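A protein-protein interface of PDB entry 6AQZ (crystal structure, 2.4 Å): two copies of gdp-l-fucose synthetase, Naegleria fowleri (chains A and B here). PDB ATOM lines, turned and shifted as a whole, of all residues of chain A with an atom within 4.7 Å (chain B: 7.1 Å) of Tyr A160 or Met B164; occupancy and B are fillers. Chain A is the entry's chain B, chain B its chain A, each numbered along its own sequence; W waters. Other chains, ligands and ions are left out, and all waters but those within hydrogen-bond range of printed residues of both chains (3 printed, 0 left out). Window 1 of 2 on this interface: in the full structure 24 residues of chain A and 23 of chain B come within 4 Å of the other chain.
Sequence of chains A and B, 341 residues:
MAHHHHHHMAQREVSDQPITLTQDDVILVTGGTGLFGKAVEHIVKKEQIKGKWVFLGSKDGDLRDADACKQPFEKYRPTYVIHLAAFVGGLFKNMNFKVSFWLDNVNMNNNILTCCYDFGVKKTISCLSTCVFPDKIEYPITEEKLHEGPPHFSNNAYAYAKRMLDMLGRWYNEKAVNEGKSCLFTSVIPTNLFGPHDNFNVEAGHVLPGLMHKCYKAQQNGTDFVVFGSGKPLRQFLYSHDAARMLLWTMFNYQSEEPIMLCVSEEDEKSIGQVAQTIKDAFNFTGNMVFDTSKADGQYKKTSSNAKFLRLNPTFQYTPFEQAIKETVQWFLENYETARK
NE1 of Trp A102 lies within hydrogen-bond range of OD1 of Asn B110, 3.1 Å away.
OD1 of Asn A156 is in hydrogen-bond range of NE1 of Trp B171 (3.0 Å).
A ring nitrogen (NE2) of His B147 lies within hydrogen-bond range of the side-chain sulfur (SD) of Met B167 (3.8 Å).
The backbone carbonyl oxygen (O) of Val B106 lies close to the side-chain amide nitrogen (ND2) of Asn B110 (3.2 Å).
NE2 of His B147 sits at hydrogen-bond distance from OD2 of Asp B166, 2.8 Å away.
Trp A102 touches Val B106 (CZ2 to CG2, 3.9 Å).
Trp A102 touches Met B164 (CH2 to CG, 3.5 Å).
CD1 of Trp A102 touches CD1 of Leu B168, 3.97 Å away.
CG of Trp A102 touches CZ3 of Trp B171 (3.6 Å).
His B147 touches Pro A150 (O to CD, 3.5 Å).
Glu B148 touches Pro A150 (OE2 to CG, 3.7 Å).
Met B167 touches Asn A156 (CE to ND2, 3.4 Å).
CD1 of Tyr A160 touches CE of Met B164, at 3.6 Å.
Met B167 touches Tyr A160.
Met A164 touches Tyr B160.
Met B164 touches just these residues of chain A: Trp A102 (3.5 Å) and Tyr A160 (3.6 Å).
Of the printed residues of chain A, Glu B148 touches Pro A150 (3.7 Å).
Printed residues of chain A within 4 Å of Met B167: Asn A156 (3.4 Å) and Tyr A160 (3.999 Å).
Leu B165 touches none of the printed residues of chain A.
Ala B161 touches none of the printed residues of chain A.
The nearest printed residue of chain B that does not touch Tyr A160 is Trp B171 (4.1 Å).
The nearest printed residue of chain A that does not touch Met B167 is Ala A157 (6.2 Å).
Of the 12 printed residues of chain A, 6 touch a printed residue of chain B.
Hydrophobic or aromatic side chains of chain A within 4 Å of the printed part of chain B: Trp A102, Pro A150, Ala A157, Tyr A160 and Met A164.
Of the 22 printed residues of chain B, 10 touch a printed residue of chain A.
Printed residues of chain B that touch a printed residue of chain A: Trp B102, Val B106, Asn B110, His B147, Glu B148, Tyr B160, Met B164, Met B167, Leu B168 and Trp B171.
Hydrophobic or aromatic side chains of chain B that line the printed part of chain A: Trp B102, Val B106, His B147, Tyr B160, Met B164, Met B167, Leu B168 and Trp B171.
Along chain B the printed residues that touch a printed residue of chain A span positions 102 to 171.
Among the printed residues, no Asp or Glu carboxylate lies within 4 Å of a Lys or Arg side-chain nitrogen of the other chain.
Trp A102 touches Met B164, and with the chains exchanged Met A164 touches Trp B102.
Tyr A160 touches Met B164, and with the chains exchanged Met A164 touches Tyr B160.
Water W2 lies within hydrogen-bond range of the backbone carbonyl oxygen of His B147 and the side-chain hydroxyl of Tyr A160.
Water W3 bridges ND2 of Asn A156 (2.8 Å) and NE1 of Trp B171 (3.5 Å).
Water W1 lies within hydrogen-bond range of a ring nitrogen (ND1) of His B147 (2.8 Å), the guanidinium group of Arg B163 (3.1 Å) and the side-chain hydroxyl of Tyr A160 (3.5 Å).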
ATOM      1  N   TRP A 102      35.802  19.297   2.998  1.00  0.00           N
ATOM      2  CA  TRP A 102      34.605  19.110   3.821  1.00  0.00           C
ATOM      3  C   TRP A 102      34.930  19.363   5.297  1.00  0.00           C
ATOM      4  O   TRP A 102      34.304  20.206   5.944  1.00  0.00           O
ATOM      5  CB  TRP A 102      33.994  17.705   3.607  1.00  0.00           C
ATOM      6  CG  TRP A 102      32.966  17.393   4.670  1.00  0.00           C
ATOM      7  CD1 TRP A 102      33.122  16.530   5.719  1.00  0.00           C
ATOM      8  CD2 TRP A 102      31.647  17.972   4.821  1.00  0.00           C
ATOM      9  NE1 TRP A 102      31.998  16.539   6.507  1.00  0.00           N
ATOM     10  CE2 TRP A 102      31.082  17.417   5.985  1.00  0.00           C
ATOM     11  CE3 TRP A 102      30.899  18.901   4.089  1.00  0.00           C
ATOM     12  CZ2 TRP A 102      29.793  17.757   6.434  1.00  0.00           C
ATOM     13  CZ3 TRP A 102      29.625  19.237   4.530  1.00  0.00           C
ATOM     14  CH2 TRP A 102      29.082  18.668   5.697  1.00  0.00           C
ATOM     15  N   PRO A 150      21.465  18.356  -5.940  1.00  0.00           N
ATOM     16  CA  PRO A 150      22.882  18.267  -5.576  1.00  0.00           C
ATOM     17  C   PRO A 150      23.716  19.269  -6.351  1.00  0.00           C
ATOM     18  O   PRO A 150      23.404  19.605  -7.508  1.00  0.00           O
ATOM     19  CB  PRO A 150      23.250  16.816  -5.950  1.00  0.00           C
ATOM     20  CG  PRO A 150      22.291  16.467  -7.054  1.00  0.00           C
ATOM     21  CD  PRO A 150      21.016  17.192  -6.736  1.00  0.00           C
ATOM     22  N   PRO A 151      24.795  19.779  -5.762  1.00  0.00           N
ATOM     23  CA  PRO A 151      25.673  20.686  -6.519  1.00  0.00           C
ATOM     24  C   PRO A 151      26.459  19.887  -7.535  1.00  0.00           C
ATOM     25  O   PRO A 151      26.359  18.657  -7.575  1.00  0.00           O
ATOM     26  CB  PRO A 151      26.589  21.277  -5.448  1.00  0.00           C
ATOM     27  CG  PRO A 151      26.707  20.135  -4.458  1.00  0.00           C
ATOM     28  CD  PRO A 151      25.346  19.448  -4.439  1.00  0.00           C
ATOM     29  N   ASN A 156      31.835  19.438  -4.858  1.00  0.00           N
ATOM     30  CA  ASN A 156      30.652  19.237  -4.031  1.00  0.00           C
ATOM     31  C   ASN A 156      30.980  19.226  -2.539  1.00  0.00           C
ATOM     32  O   ASN A 156      30.096  19.531  -1.741  1.00  0.00           O
ATOM     33  CB  ASN A 156      29.858  17.986  -4.464  1.00  0.00           C
ATOM     34  CG  ASN A 156      30.646  16.678  -4.398  1.00  0.00           C
ATOM     35  OD1 ASN A 156      31.808  16.627  -4.002  1.00  0.00           O
ATOM     36  ND2 ASN A 156      29.984  15.606  -4.782  1.00  0.00           N
ATOM     37  N   ALA A 157      32.235  18.971  -2.150  1.00  0.00           N
ATOM     38  CA  ALA A 157      32.608  19.044  -0.733  1.00  0.00           C
ATOM     39  C   ALA A 157      32.564  20.469  -0.216  1.00  0.00           C
ATOM     40  O   ALA A 157      31.951  20.743   0.823  1.00  0.00           O
ATOM     41  CB  ALA A 157      34.000  18.448  -0.512  1.00  0.00           C
ATOM     42  N   TYR A 158      33.241  21.385  -0.916  1.00  0.00           N
ATOM     43  CA  TYR A 158      33.122  22.806  -0.608  1.00  0.00           C
ATOM     44  C   TYR A 158      31.662  23.247  -0.675  1.00  0.00           C
ATOM     45  O   TYR A 158      31.178  23.955   0.215  1.00  0.00           O
ATOM     46  CB  TYR A 158      33.995  23.623  -1.586  1.00  0.00           C
ATOM     47  CG  TYR A 158      33.853  25.127  -1.469  1.00  0.00           C
ATOM     48  CD1 TYR A 158      34.637  25.867  -0.587  1.00  0.00           C
ATOM     49  CD2 TYR A 158      32.907  25.806  -2.218  1.00  0.00           C
ATOM     50  CE1 TYR A 158      34.485  27.243  -0.468  1.00  0.00           C
ATOM     51  CE2 TYR A 158      32.752  27.182  -2.112  1.00  0.00           C
ATOM     52  CZ  TYR A 158      33.539  27.891  -1.234  1.00  0.00           C
ATOM     53  OH  TYR A 158      33.364  29.243  -1.124  1.00  0.00           O
ATOM     54  N   ALA A 159      30.927  22.782  -1.694  1.00  0.00           N
ATOM     55  CA  ALA A 159      29.553  23.238  -1.888  1.00  0.00           C
ATOM     56  C   ALA A 159      28.654  22.824  -0.733  1.00  0.00           C
ATOM     57  O   ALA A 159      27.930  23.661  -0.174  1.00  0.00           O
ATOM     58  CB  ALA A 159      28.999  22.687  -3.193  1.00  0.00           C
ATOM     59  N   TYR A 160      28.723  21.541  -0.330  1.00  0.00           N
ATOM     60  CA  TYR A 160      27.866  21.060   0.743  1.00  0.00           C
ATOM     61  C   TYR A 160      28.219  21.722   2.079  1.00  0.00           C
ATOM     62  O   TYR A 160      27.326  22.103   2.842  1.00  0.00           O
ATOM     63  CB  TYR A 160      27.960  19.534   0.824  1.00  0.00           C
ATOM     64  CG  TYR A 160      26.974  18.815  -0.071  1.00  0.00           C
ATOM     65  CD1 TYR A 160      25.624  19.110   0.001  1.00  0.00           C
ATOM     66  CD2 TYR A 160      27.385  17.834  -0.975  1.00  0.00           C
ATOM     67  CE1 TYR A 160      24.711  18.464  -0.797  1.00  0.00           C
ATOM     68  CE2 TYR A 160      26.464  17.183  -1.796  1.00  0.00           C
ATOM     69  CZ  TYR A 160      25.125  17.504  -1.687  1.00  0.00           C
ATOM     70  OH  TYR A 160      24.174  16.875  -2.460  1.00  0.00           O
ATOM     71  N   ALA A 161      29.513  21.921   2.352  1.00  0.00           N
ATOM     72  CA  ALA A 161      29.891  22.661   3.551  1.00  0.00           C
ATOM     73  C   ALA A 161      29.268  24.057   3.555  1.00  0.00           C
ATOM     74  O   ALA A 161      28.803  24.525   4.594  1.00  0.00           O
ATOM     75  CB  ALA A 161      31.417  22.738   3.667  1.00  0.00           C
ATOM     76  N   LYS A 162      29.233  24.736   2.401  1.00  0.00           N
ATOM     77  CA  LYS A 162      28.521  26.014   2.336  1.00  0.00           C
ATOM     78  C   LYS A 162      27.011  25.831   2.519  1.00  0.00           C
ATOM     79  O   LYS A 162      26.347  26.653   3.168  1.00  0.00           O
ATOM     80  CB  LYS A 162      28.805  26.733   1.016  1.00  0.00           C
ATOM     81  CG  LYS A 162      30.195  27.327   0.888  1.00  0.00           C
ATOM     82  CD  LYS A 162      30.476  28.279   2.044  1.00  0.00           C
ATOM     83  CE  LYS A 162      31.568  29.304   1.635  1.00  0.00           C
ATOM     84  NZ  LYS A 162      31.951  30.174   2.775  1.00  0.00           N
ATOM     85  N   ARG A 163      26.442  24.781   1.925  1.00  0.00           N
ATOM     86  CA  ARG A 163      25.025  24.519   2.139  1.00  0.00           C
ATOM     87  C   ARG A 163      24.720  24.380   3.633  1.00  0.00           C
ATOM     88  O   ARG A 163      23.730  24.933   4.137  1.00  0.00           O
ATOM     89  CB  ARG A 163      24.622  23.243   1.405  1.00  0.00           C
ATOM     90  CG  ARG A 163      24.835  23.252  -0.135  1.00  0.00           C
ATOM     91  CD  ARG A 163      23.579  23.541  -0.902  1.00  0.00           C
ATOM     92  NE  ARG A 163      23.725  23.294  -2.336  1.00  0.00           N
ATOM     93  CZ  ARG A 163      23.145  22.305  -3.022  1.00  0.00           C
ATOM     94  NH1 ARG A 163      22.337  21.417  -2.428  1.00  0.00           N
ATOM     95  NH2 ARG A 163      23.361  22.214  -4.329  1.00  0.00           N
ATOM     96  N   MET A 164      25.564  23.647   4.357  1.00  0.00           N
ATOM     97  CA  MET A 164      25.351  23.427   5.784  1.00  0.00           C
ATOM     98  C   MET A 164      25.721  24.651   6.624  1.00  0.00           C
ATOM     99  O   MET A 164      25.262  24.777   7.756  1.00  0.00           O
ATOM    100  CB  MET A 164      26.116  22.171   6.219  1.00  0.00           C
ATOM    101  CG  MET A 164      25.596  20.891   5.519  1.00  0.00           C
ATOM    102  SD  MET A 164      23.792  20.700   5.644  1.00  0.00           S
ATOM    103  CE  MET A 164      23.251  21.043   3.981  1.00  0.00           C
ATOM    104  N   TRP B 102      22.262  18.380  14.359  1.00  0.00           N
ATOM    105  CA  TRP B 102      23.306  18.557  13.356  1.00  0.00           C
ATOM    106  C   TRP B 102      24.687  18.292  13.958  1.00  0.00           C
ATOM    107  O   TRP B 102      25.424  17.418  13.493  1.00  0.00           O
ATOM    108  CB  TRP B 102      23.256  19.959  12.742  1.00  0.00           C
ATOM    109  CG  TRP B 102      24.458  20.206  11.890  1.00  0.00           C
ATOM    110  CD1 TRP B 102      25.515  21.009  12.185  1.00  0.00           C
ATOM    111  CD2 TRP B 102      24.757  19.584  10.629  1.00  0.00           C
ATOM    112  NE1 TRP B 102      26.446  20.941  11.185  1.00  0.00           N
ATOM    113  CE2 TRP B 102      26.010  20.074  10.214  1.00  0.00           C
ATOM    114  CE3 TRP B 102      24.071  18.680   9.803  1.00  0.00           C
ATOM    115  CZ2 TRP B 102      26.606  19.707   8.988  1.00  0.00           C
ATOM    116  CZ3 TRP B 102      24.675  18.279   8.613  1.00  0.00           C
ATOM    117  CH2 TRP B 102      25.929  18.810   8.205  1.00  0.00           C
ATOM    118  N   VAL B 106      27.013  15.195  13.009  1.00  0.00           N
ATOM    119  CA  VAL B 106      28.065  15.410  12.026  1.00  0.00           C
ATOM    120  C   VAL B 106      29.439  15.236  12.683  1.00  0.00           C
ATOM    121  O   VAL B 106      30.383  14.749  12.040  1.00  0.00           O
ATOM    122  CB  VAL B 106      27.919  16.774  11.314  1.00  0.00           C
ATOM    123  CG1 VAL B 106      28.465  17.967  12.179  1.00  0.00           C
ATOM    124  CG2 VAL B 106      28.601  16.692   9.962  1.00  0.00           C
ATOM    125  N   ASN B 109      29.949  11.412  13.055  1.00  0.00           N
ATOM    126  CA  ASN B 109      30.195  10.800  11.745  1.00  0.00           C
ATOM    127  C   ASN B 109      31.567  11.171  11.190  1.00  0.00           C
ATOM    128  O   ASN B 109      32.304  10.301  10.711  1.00  0.00           O
ATOM    129  CB  ASN B 109      29.074  11.161  10.781  1.00  0.00           C
ATOM    130  CG  ASN B 109      27.788  10.475  11.145  1.00  0.00           C
ATOM    131  OD1 ASN B 109      27.822   9.414  11.761  1.00  0.00           O
ATOM    132  ND2 ASN B 109      26.652  11.060  10.784  1.00  0.00           N
ATOM    133  N   ASN B 110      31.936  12.451  11.258  1.00  0.00           N
ATOM    134  CA  ASN B 110      33.268  12.848  10.803  1.00  0.00           C
ATOM    135  C   ASN B 110      34.362  12.097  11.571  1.00  0.00           C
ATOM    136  O   ASN B 110      35.315  11.583  10.967  1.00  0.00           O
ATOM    137  CB  ASN B 110      33.435  14.378  10.915  1.00  0.00           C
ATOM    138  CG  ASN B 110      32.560  15.138   9.892  1.00  0.00           C
ATOM    139  OD1 ASN B 110      32.051  14.547   8.925  1.00  0.00           O
ATOM    140  ND2 ASN B 110      32.339  16.434  10.137  1.00  0.00           N
ATOM    141  N   LEU B 113      34.415   7.982  10.568  1.00  0.00           N
ATOM    142  CA  LEU B 113      34.941   7.696   9.225  1.00  0.00           C
ATOM    143  C   LEU B 113      36.399   8.114   9.104  1.00  0.00           C
ATOM    144  O   LEU B 113      37.194   7.429   8.463  1.00  0.00           O
ATOM    145  CB  LEU B 113      34.118   8.382   8.131  1.00  0.00           C
ATOM    146  CG  LEU B 113      32.980   7.493   7.575  1.00  0.00           C
ATOM    147  CD1 LEU B 113      32.074   6.988   8.699  1.00  0.00           C
ATOM    148  CD2 LEU B 113      32.155   8.209   6.517  1.00  0.00           C
ATOM    149  N   LEU B 128      22.130   4.822   7.313  1.00  0.00           N
ATOM    150  CA  LEU B 128      21.237   5.934   7.015  1.00  0.00           C
ATOM    151  C   LEU B 128      19.824   5.568   7.472  1.00  0.00           C
ATOM    152  O   LEU B 128      19.639   4.700   8.327  1.00  0.00           O
ATOM    153  CB  LEU B 128      21.256   6.290   5.522  1.00  0.00           C
ATOM    154  CG  LEU B 128      22.613   6.401   4.835  1.00  0.00           C
ATOM    155  CD1 LEU B 128      22.478   6.878   3.382  1.00  0.00           C
ATOM    156  CD2 LEU B 128      23.575   7.243   5.603  1.00  0.00           C
ATOM    157  N   HIS B 147      19.781  12.503  -2.649  1.00  0.00           N
ATOM    158  CA  HIS B 147      20.174  13.917  -2.590  1.00  0.00           C
ATOM    159  C   HIS B 147      19.381  14.797  -3.544  1.00  0.00           C
ATOM    160  O   HIS B 147      19.747  15.958  -3.756  1.00  0.00           O
ATOM    161  CB  HIS B 147      21.668  14.076  -2.892  1.00  0.00           C
ATOM    162  CG  HIS B 147      22.555  13.283  -1.987  1.00  0.00           C
ATOM    163  ND1 HIS B 147      22.892  13.698  -0.715  1.00  0.00           N
ATOM    164  CD2 HIS B 147      23.187  12.102  -2.176  1.00  0.00           C
ATOM    165  CE1 HIS B 147      23.677  12.797  -0.150  1.00  0.00           C
ATOM    166  NE2 HIS B 147      23.868  11.815  -1.011  1.00  0.00           N
ATOM    167  N   GLU B 148      18.294  14.290  -4.112  1.00  0.00           N
ATOM    168  CA  GLU B 148      17.559  15.011  -5.150  1.00  0.00           C
ATOM    169  C   GLU B 148      16.516  15.938  -4.518  1.00  0.00           C
ATOM    170  O   GLU B 148      15.318  15.850  -4.787  1.00  0.00           O
ATOM    171  CB  GLU B 148      16.897  14.022  -6.100  1.00  0.00           C
ATOM    172  CG  GLU B 148      17.905  13.124  -6.833  1.00  0.00           C
ATOM    173  CD  GLU B 148      18.920  13.890  -7.675  1.00  0.00           C
ATOM    174  OE1 GLU B 148      18.548  14.888  -8.327  1.00  0.00           O
ATOM    175  OE2 GLU B 148      20.109  13.503  -7.655  1.00  0.00           O
ATOM    176  N   TYR B 158      18.829  16.162  11.441  1.00  0.00           N
ATOM    177  CA  TYR B 158      19.177  14.752  11.434  1.00  0.00           C
ATOM    178  C   TYR B 158      19.304  14.245   9.998  1.00  0.00           C
ATOM    179  O   TYR B 158      20.266  13.552   9.657  1.00  0.00           O
ATOM    180  CB  TYR B 158      18.115  13.981  12.225  1.00  0.00           C
ATOM    181  CG  TYR B 158      18.298  12.500  12.262  1.00  0.00           C
ATOM    182  CD1 TYR B 158      19.110  11.921  13.225  1.00  0.00           C
ATOM    183  CD2 TYR B 158      17.647  11.668  11.357  1.00  0.00           C
ATOM    184  CE1 TYR B 158      19.278  10.555  13.294  1.00  0.00           C
ATOM    185  CE2 TYR B 158      17.811  10.288  11.422  1.00  0.00           C
ATOM    186  CZ  TYR B 158      18.636   9.746  12.397  1.00  0.00           C
ATOM    187  OH  TYR B 158      18.827   8.394  12.490  1.00  0.00           O
ATOM    188  N   ALA B 159      18.373  14.626   9.130  1.00  0.00           N
ATOM    189  CA  ALA B 159      18.409  14.093   7.778  1.00  0.00           C
ATOM    190  C   ALA B 159      19.682  14.533   7.049  1.00  0.00           C
ATOM    191  O   ALA B 159      20.360  13.714   6.424  1.00  0.00           O
ATOM    192  CB  ALA B 159      17.155  14.527   7.020  1.00  0.00           C
ATOM    193  N   TYR B 160      20.047  15.821   7.156  1.00  0.00           N
ATOM    194  CA  TYR B 160      21.236  16.308   6.459  1.00  0.00           C
ATOM    195  C   TYR B 160      22.509  15.683   7.009  1.00  0.00           C
ATOM    196  O   TYR B 160      23.422  15.355   6.239  1.00  0.00           O
ATOM    197  CB  TYR B 160      21.316  17.840   6.526  1.00  0.00           C
ATOM    198  CG  TYR B 160      20.563  18.530   5.408  1.00  0.00           C
ATOM    199  CD1 TYR B 160      20.802  18.201   4.069  1.00  0.00           C
ATOM    200  CD2 TYR B 160      19.609  19.495   5.687  1.00  0.00           C
ATOM    201  CE1 TYR B 160      20.115  18.836   3.055  1.00  0.00           C
ATOM    202  CE2 TYR B 160      18.930  20.134   4.681  1.00  0.00           C
ATOM    203  CZ  TYR B 160      19.180  19.806   3.372  1.00  0.00           C
ATOM    204  OH  TYR B 160      18.465  20.450   2.380  1.00  0.00           O
ATOM    205  N   ALA B 161      22.582  15.487   8.329  1.00  0.00           N
ATOM    206  CA  ALA B 161      23.732  14.787   8.899  1.00  0.00           C
ATOM    207  C   ALA B 161      23.886  13.387   8.301  1.00  0.00           C
ATOM    208  O   ALA B 161      25.009  12.949   8.005  1.00  0.00           O
ATOM    209  CB  ALA B 161      23.600  14.718  10.419  1.00  0.00           C
ATOM    210  N   LYS B 162      22.769  12.681   8.084  1.00  0.00           N
ATOM    211  CA  LYS B 162      22.852  11.367   7.443  1.00  0.00           C
ATOM    212  C   LYS B 162      23.320  11.490   5.993  1.00  0.00           C
ATOM    213  O   LYS B 162      24.151  10.696   5.527  1.00  0.00           O
ATOM    214  CB  LYS B 162      21.504  10.636   7.517  1.00  0.00           C
ATOM    215  CG  LYS B 162      21.125  10.162   8.880  1.00  0.00           C
ATOM    216  CD  LYS B 162      22.183   9.260   9.465  1.00  0.00           C
ATOM    217  CE  LYS B 162      21.646   8.325  10.598  1.00  0.00           C
ATOM    218  NZ  LYS B 162      22.861   7.577  11.168  1.00  0.00           N
ATOM    219  N   ARG B 163      22.801  12.482   5.268  1.00  0.00           N
ATOM    220  CA  ARG B 163      23.263  12.725   3.902  1.00  0.00           C
ATOM    221  C   ARG B 163      24.765  12.987   3.839  1.00  0.00           C
ATOM    222  O   ARG B 163      25.447  12.495   2.926  1.00  0.00           O
ATOM    223  CB  ARG B 163      22.499  13.898   3.279  1.00  0.00           C
ATOM    224  CG  ARG B 163      21.033  13.601   3.161  1.00  0.00           C
ATOM    225  CD  ARG B 163      20.422  14.587   2.278  1.00  0.00           C
ATOM    226  NE  ARG B 163      18.997  14.372   2.112  1.00  0.00           N
ATOM    227  CZ  ARG B 163      18.279  15.024   1.211  1.00  0.00           C
ATOM    228  NH1 ARG B 163      18.901  15.889   0.408  1.00  0.00           N
ATOM    229  NH2 ARG B 163      16.972  14.809   1.105  1.00  0.00           N
ATOM    230  N   MET B 164      25.289  13.790   4.771  1.00  0.00           N
ATOM    231  CA  MET B 164      26.716  14.099   4.775  1.00  0.00           C
ATOM    232  C   MET B 164      27.571  12.923   5.260  1.00  0.00           C
ATOM    233  O   MET B 164      28.761  12.867   4.932  1.00  0.00           O
ATOM    234  CB  MET B 164      26.945  15.360   5.616  1.00  0.00           C
ATOM    235  CG  MET B 164      26.282  16.628   5.015  1.00  0.00           C
ATOM    236  SD  MET B 164      26.729  16.883   3.252  1.00  0.00           S
ATOM    237  CE  MET B 164      25.205  16.468   2.408  1.00  0.00           C
ATOM    238  N   LEU B 165      26.982  11.968   5.991  1.00  0.00           N
ATOM    239  CA  LEU B 165      27.665  10.707   6.283  1.00  0.00           C
ATOM    240  C   LEU B 165      27.857   9.891   5.006  1.00  0.00           C
ATOM    241  O   LEU B 165      28.936   9.329   4.772  1.00  0.00           O
ATOM    242  CB  LEU B 165      26.886   9.920   7.354  1.00  0.00           C
ATOM    243  CG  LEU B 165      27.113   8.420   7.654  1.00  0.00           C
ATOM    244  CD1 LEU B 165      28.559   8.136   8.029  1.00  0.00           C
ATOM    245  CD2 LEU B 165      26.187   7.955   8.821  1.00  0.00           C
ATOM    246  N   ASP B 166      26.821   9.832   4.172  1.00  0.00           N
ATOM    247  CA  ASP B 166      26.941   9.195   2.873  1.00  0.00           C
ATOM    248  C   ASP B 166      27.997   9.891   2.017  1.00  0.00           C
ATOM    249  O   ASP B 166      28.857   9.221   1.418  1.00  0.00           O
ATOM    250  CB  ASP B 166      25.582   9.184   2.172  1.00  0.00           C
ATOM    251  CG  ASP B 166      25.694   8.789   0.690  1.00  0.00           C
ATOM    252  OD1 ASP B 166      26.107   7.652   0.412  1.00  0.00           O
ATOM    253  OD2 ASP B 166      25.358   9.610  -0.197  1.00  0.00           O
ATOM    254  N   MET B 167      27.957  11.240   1.951  1.00  0.00           N
ATOM    255  CA  MET B 167      28.931  11.960   1.116  1.00  0.00           C
ATOM    256  C   MET B 167      30.344  11.772   1.643  1.00  0.00           C
ATOM    257  O   MET B 167      31.265  11.503   0.870  1.00  0.00           O
ATOM    258  CB  MET B 167      28.628  13.461   1.020  1.00  0.00           C
ATOM    259  CG  MET B 167      27.405  13.845   0.196  1.00  0.00           C
ATOM    260  SD  MET B 167      27.396  13.105  -1.463  1.00  0.00           S
ATOM    261  CE  MET B 167      28.937  13.715  -2.169  1.00  0.00           C
ATOM    262  N   LEU B 168      30.529  11.851   2.964  1.00  0.00           N
ATOM    263  CA  LEU B 168      31.876  11.713   3.505  1.00  0.00           C
ATOM    264  C   LEU B 168      32.485  10.363   3.146  1.00  0.00           C
ATOM    265  O   LEU B 168      33.690  10.275   2.879  1.00  0.00           O
ATOM    266  CB  LEU B 168      31.862  11.905   5.026  1.00  0.00           C
ATOM    267  CG  LEU B 168      33.281  11.846   5.619  1.00  0.00           C
ATOM    268  CD1 LEU B 168      34.235  12.810   4.899  1.00  0.00           C
ATOM    269  CD2 LEU B 168      33.255  12.106   7.134  1.00  0.00           C
ATOM    270  N   GLY B 169      31.661   9.304   3.112  1.00  0.00           N
ATOM    271  CA  GLY B 169      32.146   8.000   2.678  1.00  0.00           C
ATOM    272  C   GLY B 169      32.593   8.006   1.222  1.00  0.00           C
ATOM    273  O   GLY B 169      33.598   7.386   0.860  1.00  0.00           O
ATOM    274  N   ARG B 170      31.822   8.667   0.357  1.00  0.00           N
ATOM    275  CA  ARG B 170      32.224   8.729  -1.041  1.00  0.00           C
ATOM    276  C   ARG B 170      33.555   9.460  -1.183  1.00  0.00           C
ATOM    277  O   ARG B 170      34.445   9.015  -1.917  1.00  0.00           O
ATOM    278  CB  ARG B 170      31.134   9.414  -1.859  1.00  0.00           C
ATOM    279  CG  ARG B 170      29.772   8.750  -1.757  1.00  0.00           C
ATOM    280  CD  ARG B 170      28.739   9.618  -2.464  1.00  0.00           C
ATOM    281  NE  ARG B 170      27.388   9.117  -2.282  1.00  0.00           N
ATOM    282  CZ  ARG B 170      26.742   8.353  -3.154  1.00  0.00           C
ATOM    283  NH1 ARG B 170      27.332   8.000  -4.316  1.00  0.00           N
ATOM    284  NH2 ARG B 170      25.498   7.968  -2.874  1.00  0.00           N
ATOM    285  N   TRP B 171      33.726  10.544  -0.424  1.00  0.00           N
ATOM    286  CA  TRP B 171      34.956  11.320  -0.474  1.00  0.00           C
ATOM    287  C   TRP B 171      36.131  10.528   0.095  1.00  0.00           C
ATOM    288  O   TRP B 171      37.241  10.591  -0.440  1.00  0.00           O
ATOM    289  CB  TRP B 171      34.750  12.633   0.288  1.00  0.00           C
ATOM    290  CG  TRP B 171      33.733  13.513  -0.360  1.00  0.00           C
ATOM    291  CD1 TRP B 171      33.485  13.616  -1.701  1.00  0.00           C
ATOM    292  CD2 TRP B 171      32.803  14.400   0.288  1.00  0.00           C
ATOM    293  NE1 TRP B 171      32.479  14.518  -1.927  1.00  0.00           N
ATOM    294  CE2 TRP B 171      32.042  15.019  -0.729  1.00  0.00           C
ATOM    295  CE3 TRP B 171      32.540  14.727   1.624  1.00  0.00           C
ATOM    296  CZ2 TRP B 171      31.048  15.956  -0.459  1.00  0.00           C
ATOM    297  CZ3 TRP B 171      31.545  15.653   1.893  1.00  0.00           C
ATOM    298  CH2 TRP B 171      30.809  16.255   0.855  1.00  0.00           C
HETATM  299  O   HOH W   1      21.935  16.231   0.143  1.00  0.00           O
HETATM  300  O   HOH W   2      21.150  17.907  -2.429  1.00  0.00           O
HETATM  301  O   HOH W   3      31.518  13.284  -5.011  1.00  0.00           O
